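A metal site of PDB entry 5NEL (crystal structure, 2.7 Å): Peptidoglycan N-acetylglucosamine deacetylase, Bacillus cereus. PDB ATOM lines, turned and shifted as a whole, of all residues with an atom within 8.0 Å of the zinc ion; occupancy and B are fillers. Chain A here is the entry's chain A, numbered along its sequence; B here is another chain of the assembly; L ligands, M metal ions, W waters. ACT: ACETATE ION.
The side-chain carboxylate of Asp 50 is in salt-bridge range of the guanidinium group of Arg 138, at 2.7 Å. O of Met 203 sits at hydrogen-bond distance from N of Asp 50 (2.8 Å). The backbone NH (N) of Asp 51 lies within hydrogen-bond range of the backbone carbonyl oxygen (O) of Phe 74 (3.4 Å). NE2 of His 100 lies close to OD2 of Asp 50 (3.4 Å). ND1 of His 100 sits at hydrogen-bond distance from O of Arg 138, 2.6 Å away. O of His 104 sits at hydrogen-bond distance from OH of Tyr 141 (3.2 Å). The side-chain hydroxyl (OG) of Ser 101 sits at hydrogen-bond distance from the backbone NH (N) of His 104 (3.0 Å).
Merely in contact with the zinc ion: Asp 50 (3.7 Å). Within 4 Å of the zinc ion: Asp 50, Asp 51, His 100 and His 104. Along chain A the residues within 4 Å of the zinc ion span positions 50 to 104. The nearest printed residue that does not touch the zinc ion is Pro 140 (4.6 Å).
The zinc ion is bound by water W1 (2.1 Å), the side-chain carboxylate of Asp 51 (2.1 Å), a ring nitrogen (NE2) of His 104 (2.1 Å), a ring nitrogen (NE2) of His 100 (2.3 Å), an oxygen (O) of the ligand (2.4 Å) and an oxygen (OXT) of the ligand (2.6 Å). The zinc ion has six donor atoms within binding distance.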
ATOM      1  N   PHE A  49      15.229   6.030   2.195  1.00  0.00           N
ATOM      2  CA  PHE A  49      15.676   4.882   1.423  1.00  0.00           C
ATOM      3  C   PHE A  49      14.680   3.740   1.499  1.00  0.00           C
ATOM      4  O   PHE A  49      14.222   3.378   2.586  1.00  0.00           O
ATOM      5  CB  PHE A  49      17.054   4.412   1.900  1.00  0.00           C
ATOM      6  CG  PHE A  49      18.133   5.461   1.829  1.00  0.00           C
ATOM      7  CD1 PHE A  49      18.335   6.334   2.895  1.00  0.00           C
ATOM      8  CD2 PHE A  49      18.929   5.588   0.701  1.00  0.00           C
ATOM      9  CE1 PHE A  49      19.313   7.304   2.835  1.00  0.00           C
ATOM     10  CE2 PHE A  49      19.916   6.569   0.630  1.00  0.00           C
ATOM     11  CZ  PHE A  49      20.108   7.432   1.698  1.00  0.00           C
ATOM     12  N   ASP A  50      14.398   3.140   0.333  1.00  0.00           N
ATOM     13  CA  ASP A  50      13.363   2.109   0.214  1.00  0.00           C
ATOM     14  C   ASP A  50      13.882   0.690   0.013  1.00  0.00           C
ATOM     15  O   ASP A  50      15.041   0.472  -0.362  1.00  0.00           O
ATOM     16  CB  ASP A  50      12.428   2.419  -0.963  1.00  0.00           C
ATOM     17  CG  ASP A  50      11.400   3.476  -0.659  1.00  0.00           C
ATOM     18  OD1 ASP A  50      11.544   4.248   0.327  1.00  0.00           O
ATOM     19  OD2 ASP A  50      10.413   3.514  -1.423  1.00  0.00           O
ATOM     20  N   ASP A  51      12.982  -0.261   0.265  1.00  0.00           N
ATOM     21  CA  ASP A  51      13.139  -1.653  -0.118  1.00  0.00           C
ATOM     22  C   ASP A  51      14.254  -2.386   0.630  1.00  0.00           C
ATOM     23  O   ASP A  51      14.564  -3.536   0.304  1.00  0.00           O
ATOM     24  CB  ASP A  51      13.399  -1.757  -1.635  1.00  0.00           C
ATOM     25  CG  ASP A  51      12.303  -1.103  -2.498  1.00  0.00           C
ATOM     26  OD1 ASP A  51      11.131  -0.928  -2.084  1.00  0.00           O
ATOM     27  OD2 ASP A  51      12.638  -0.723  -3.641  1.00  0.00           O
ATOM     28  N   GLY A  52      14.833  -1.758   1.648  1.00  0.00           N
ATOM     29  CA  GLY A  52      15.883  -2.382   2.430  1.00  0.00           C
ATOM     30  C   GLY A  52      15.457  -3.058   3.734  1.00  0.00           C
ATOM     31  O   GLY A  52      14.271  -3.258   3.978  1.00  0.00           O
ATOM     32  N   PHE A  74      12.756   2.992   5.028  1.00  0.00           N
ATOM     33  CA  PHE A  74      11.486   2.289   4.999  1.00  0.00           C
ATOM     34  C   PHE A  74      11.711   0.826   4.606  1.00  0.00           C
ATOM     35  O   PHE A  74      11.961   0.535   3.450  1.00  0.00           O
ATOM     36  CB  PHE A  74      10.509   2.962   4.023  1.00  0.00           C
ATOM     37  CG  PHE A  74      10.212   4.381   4.364  1.00  0.00           C
ATOM     38  CD1 PHE A  74       9.348   4.696   5.408  1.00  0.00           C
ATOM     39  CD2 PHE A  74      10.769   5.410   3.615  1.00  0.00           C
ATOM     40  CE1 PHE A  74       9.067   6.028   5.727  1.00  0.00           C
ATOM     41  CE2 PHE A  74      10.486   6.742   3.924  1.00  0.00           C
ATOM     42  CZ  PHE A  74       9.636   7.045   4.984  1.00  0.00           C
ATOM     43  N   ILE A  76      11.314  -3.365   4.079  1.00  0.00           N
ATOM     44  CA  ILE A  76      10.401  -4.438   3.746  1.00  0.00           C
ATOM     45  C   ILE A  76      10.504  -5.506   4.843  1.00  0.00           C
ATOM     46  O   ILE A  76      11.564  -5.697   5.413  1.00  0.00           O
ATOM     47  CB  ILE A  76      10.700  -5.014   2.325  1.00  0.00           C
ATOM     48  CG1 ILE A  76      10.565  -3.909   1.269  1.00  0.00           C
ATOM     49  CG2 ILE A  76       9.777  -6.187   1.994  1.00  0.00           C
ATOM     50  CD1 ILE A  76      10.928  -4.352  -0.191  1.00  0.00           C
ATOM     51  N   HIS A 100       7.494  -0.308   4.888  1.00  0.00           N
ATOM     52  CA  HIS A 100       7.362  -0.360   3.444  1.00  0.00           C
ATOM     53  C   HIS A 100       6.639  -1.662   3.049  1.00  0.00           C
ATOM     54  O   HIS A 100       6.841  -2.179   1.961  1.00  0.00           O
ATOM     55  CB  HIS A 100       8.749  -0.273   2.779  1.00  0.00           C
ATOM     56  CG  HIS A 100       8.722   0.174   1.346  1.00  0.00           C
ATOM     57  ND1 HIS A 100       7.997   1.269   0.918  1.00  0.00           N
ATOM     58  CD2 HIS A 100       9.338  -0.330   0.239  1.00  0.00           C
ATOM     59  CE1 HIS A 100       8.176   1.418  -0.393  1.00  0.00           C
ATOM     60  NE2 HIS A 100       8.986   0.469  -0.827  1.00  0.00           N
ATOM     61  N   SER A 101       5.857  -2.193   3.998  1.00  0.00           N
ATOM     62  CA  SER A 101       4.979  -3.370   3.792  1.00  0.00           C
ATOM     63  C   SER A 101       5.699  -4.702   3.888  1.00  0.00           C
ATOM     64  O   SER A 101       6.902  -4.769   4.095  1.00  0.00           O
ATOM     65  CB  SER A 101       4.262  -3.307   2.433  1.00  0.00           C
ATOM     66  OG  SER A 101       5.026  -4.029   1.458  1.00  0.00           O
ATOM     67  N   HIS A 104       5.415  -5.972  -0.791  1.00  0.00           N
ATOM     68  CA  HIS A 104       5.673  -5.004  -1.867  1.00  0.00           C
ATOM     69  C   HIS A 104       4.889  -5.381  -3.145  1.00  0.00           C
ATOM     70  O   HIS A 104       5.314  -5.057  -4.250  1.00  0.00           O
ATOM     71  CB  HIS A 104       7.186  -4.907  -2.155  1.00  0.00           C
ATOM     72  CG  HIS A 104       7.645  -3.553  -2.626  1.00  0.00           C
ATOM     73  ND1 HIS A 104       7.164  -2.953  -3.779  1.00  0.00           N
ATOM     74  CD2 HIS A 104       8.543  -2.679  -2.116  1.00  0.00           C
ATOM     75  CE1 HIS A 104       7.735  -1.773  -3.942  1.00  0.00           C
ATOM     76  NE2 HIS A 104       8.585  -1.581  -2.942  1.00  0.00           N
ATOM     77  N   ARG A 138       5.762   4.335   4.182  1.00  0.00           N
ATOM     78  CA  ARG A 138       6.046   4.767   2.829  1.00  0.00           C
ATOM     79  C   ARG A 138       5.456   3.717   1.913  1.00  0.00           C
ATOM     80  O   ARG A 138       5.907   2.573   1.888  1.00  0.00           O
ATOM     81  CB  ARG A 138       7.555   4.937   2.621  1.00  0.00           C
ATOM     82  CG  ARG A 138       8.074   4.568   1.281  1.00  0.00           C
ATOM     83  CD  ARG A 138       7.793   5.653   0.262  1.00  0.00           C
ATOM     84  NE  ARG A 138       8.167   6.988   0.698  1.00  0.00           N
ATOM     85  CZ  ARG A 138       9.411   7.444   0.695  1.00  0.00           C
ATOM     86  NH1 ARG A 138      10.408   6.644   0.332  1.00  0.00           N
ATOM     87  NH2 ARG A 138       9.675   8.685   1.092  1.00  0.00           N
ATOM     88  N   PRO A 139       4.390   4.092   1.210  1.00  0.00           N
ATOM     89  CA  PRO A 139       3.647   3.104   0.402  1.00  0.00           C
ATOM     90  C   PRO A 139       4.491   2.664  -0.795  1.00  0.00           C
ATOM     91  O   PRO A 139       5.071   3.495  -1.477  1.00  0.00           O
ATOM     92  CB  PRO A 139       2.396   3.872  -0.059  1.00  0.00           C
ATOM     93  CG  PRO A 139       2.713   5.317   0.092  1.00  0.00           C
ATOM     94  CD  PRO A 139       3.906   5.469   1.020  1.00  0.00           C
ATOM     95  N   PRO A 140       4.602   1.345  -0.997  1.00  0.00           N
ATOM     96  CA  PRO A 140       5.206   0.812  -2.217  1.00  0.00           C
ATOM     97  C   PRO A 140       4.514   1.384  -3.455  1.00  0.00           C
ATOM     98  O   PRO A 140       3.271   1.331  -3.553  1.00  0.00           O
ATOM     99  CB  PRO A 140       4.951  -0.692  -2.100  1.00  0.00           C
ATOM    100  CG  PRO A 140       4.881  -0.938  -0.647  1.00  0.00           C
ATOM    101  CD  PRO A 140       4.214   0.283  -0.058  1.00  0.00           C
ATOM    102  N   TYR A 141       5.304   1.951  -4.361  1.00  0.00           N
ATOM    103  CA  TYR A 141       4.832   2.541  -5.619  1.00  0.00           C
ATOM    104  C   TYR A 141       4.155   3.896  -5.446  1.00  0.00           C
ATOM    105  O   TYR A 141       3.542   4.396  -6.389  1.00  0.00           O
ATOM    106  CB  TYR A 141       3.889   1.601  -6.362  1.00  0.00           C
ATOM    107  CG  TYR A 141       4.411   0.181  -6.543  1.00  0.00           C
ATOM    108  CD1 TYR A 141       5.464  -0.087  -7.404  1.00  0.00           C
ATOM    109  CD2 TYR A 141       3.840  -0.891  -5.867  1.00  0.00           C
ATOM    110  CE1 TYR A 141       5.948  -1.377  -7.574  1.00  0.00           C
ATOM    111  CE2 TYR A 141       4.306  -2.182  -6.023  1.00  0.00           C
ATOM    112  CZ  TYR A 141       5.357  -2.428  -6.892  1.00  0.00           C
ATOM    113  OH  TYR A 141       5.829  -3.718  -7.070  1.00  0.00           O
ATOM    114  N   GLY A 142       4.308   4.497  -4.265  1.00  0.00           N
ATOM    115  CA  GLY A 142       3.648   5.756  -3.951  1.00  0.00           C
ATOM    116  C   GLY A 142       2.203   5.509  -3.579  1.00  0.00           C
ATOM    117  O   GLY A 142       1.704   4.408  -3.822  1.00  0.00           O
ATOM    118  N   TRP A 165       7.181  11.348  -1.650  1.00  0.00           N
ATOM    119  CA  TRP A 165       8.412  12.138  -1.769  1.00  0.00           C
ATOM    120  C   TRP A 165       8.198  13.404  -2.608  1.00  0.00           C
ATOM    121  O   TRP A 165       7.143  13.597  -3.199  1.00  0.00           O
ATOM    122  CB  TRP A 165       9.536  11.279  -2.368  1.00  0.00           C
ATOM    123  CG  TRP A 165       9.113  10.611  -3.626  1.00  0.00           C
ATOM    124  CD1 TRP A 165       9.349  11.028  -4.910  1.00  0.00           C
ATOM    125  CD2 TRP A 165       8.336   9.412  -3.732  1.00  0.00           C
ATOM    126  NE1 TRP A 165       8.775  10.155  -5.800  1.00  0.00           N
ATOM    127  CE2 TRP A 165       8.146   9.153  -5.105  1.00  0.00           C
ATOM    128  CE3 TRP A 165       7.785   8.515  -2.796  1.00  0.00           C
ATOM    129  CZ2 TRP A 165       7.429   8.040  -5.573  1.00  0.00           C
ATOM    130  CZ3 TRP A 165       7.069   7.412  -3.263  1.00  0.00           C
ATOM    131  CH2 TRP A 165       6.900   7.192  -4.636  1.00  0.00           C
ATOM    132  N   LEU A 202      13.584  10.336  -2.560  1.00  0.00           N
ATOM    133  CA  LEU A 202      13.400   8.897  -2.706  1.00  0.00           C
ATOM    134  C   LEU A 202      14.694   8.288  -3.220  1.00  0.00           C
ATOM    135  O   LEU A 202      15.162   8.629  -4.311  1.00  0.00           O
ATOM    136  CB  LEU A 202      12.243   8.606  -3.656  1.00  0.00           C
ATOM    137  CG  LEU A 202      12.108   7.148  -4.121  1.00  0.00           C
ATOM    138  CD1 LEU A 202      11.699   6.273  -2.933  1.00  0.00           C
ATOM    139  CD2 LEU A 202      11.155   6.970  -5.335  1.00  0.00           C
ATOM    140  N   MET A 203      15.287   7.401  -2.426  1.00  0.00           N
ATOM    141  CA  MET A 203      16.400   6.567  -2.877  1.00  0.00           C
ATOM    142  C   MET A 203      16.179   5.115  -2.485  1.00  0.00           C
ATOM    143  O   MET A 203      15.200   4.797  -1.812  1.00  0.00           O
ATOM    144  CB  MET A 203      17.732   7.066  -2.329  1.00  0.00           C
ATOM    145  CG  MET A 203      17.958   8.530  -2.640  1.00  0.00           C
ATOM    146  SD  MET A 203      19.653   9.085  -2.526  1.00  0.00           S
ATOM    147  CE  MET A 203      20.448   8.011  -3.708  1.00  0.00           C
ATOM    148  N   HIS A 204      17.039   4.231  -2.973  1.00  0.00           N
ATOM    149  CA  HIS A 204      16.951   2.821  -2.633  1.00  0.00           C
ATOM    150  C   HIS A 204      18.351   2.289  -2.248  1.00  0.00           C
ATOM    151  O   HIS A 204      19.246   2.264  -3.083  1.00  0.00           O
ATOM    152  CB  HIS A 204      16.351   2.028  -3.807  1.00  0.00           C
ATOM    153  CG  HIS A 204      15.057   2.591  -4.322  1.00  0.00           C
ATOM    154  ND1 HIS A 204      14.989   3.735  -5.090  1.00  0.00           N
ATOM    155  CD2 HIS A 204      13.783   2.160  -4.167  1.00  0.00           C
ATOM    156  CE1 HIS A 204      13.728   3.984  -5.389  1.00  0.00           C
ATOM    157  NE2 HIS A 204      12.977   3.051  -4.847  1.00  0.00           N
ATOM    158  N   ILE A 206      19.208  -0.670  -1.601  1.00  0.00           N
ATOM    159  CA  ILE A 206      19.417  -1.998  -2.131  1.00  0.00           C
ATOM    160  C   ILE A 206      20.137  -1.896  -3.492  1.00  0.00           C
ATOM    161  O   ILE A 206      20.369  -2.899  -4.166  1.00  0.00           O
ATOM    162  CB  ILE A 206      18.075  -2.755  -2.315  1.00  0.00           C
ATOM    163  CG1 ILE A 206      17.164  -2.020  -3.318  1.00  0.00           C
ATOM    164  CG2 ILE A 206      17.391  -2.895  -0.975  1.00  0.00           C
ATOM    165  CD1 ILE A 206      16.231  -2.925  -4.111  1.00  0.00           C
ATOM    166  N   HIS B 243       9.725  -0.100 -12.561  1.00  0.00           N
ATOM    167  CA  HIS B 243      11.120   0.348 -12.522  1.00  0.00           C
ATOM    168  C   HIS B 243      12.081  -0.597 -13.222  1.00  0.00           C
ATOM    169  O   HIS B 243      13.247  -0.636 -12.892  1.00  0.00           O
ATOM    170  CB  HIS B 243      11.610   0.513 -11.075  1.00  0.00           C
ATOM    171  CG  HIS B 243      10.741   1.370 -10.219  1.00  0.00           C
ATOM    172  ND1 HIS B 243      10.424   2.666 -10.542  1.00  0.00           N
ATOM    173  CD2 HIS B 243      10.127   1.113  -9.039  1.00  0.00           C
ATOM    174  CE1 HIS B 243       9.642   3.172  -9.607  1.00  0.00           C
ATOM    175  NE2 HIS B 243       9.456   2.258  -8.683  1.00  0.00           N
HETATM  176  C   ACT L   1       9.028   2.595  -4.659  1.00  0.00           C
HETATM  177  O   ACT L   1      10.108   2.398  -4.042  1.00  0.00           O
HETATM  178  OXT ACT L   1       8.064   1.882  -4.267  1.00  0.00           O
HETATM  179  CH3 ACT L   1       8.902   3.604  -5.768  1.00  0.00           C
HETATM  180 ZN    ZN M   1       9.658   0.272  -2.999  1.00  0.00          ZN
HETATM  181  O   HOH W   1      10.632   0.043  -4.824  1.00  0.00           O
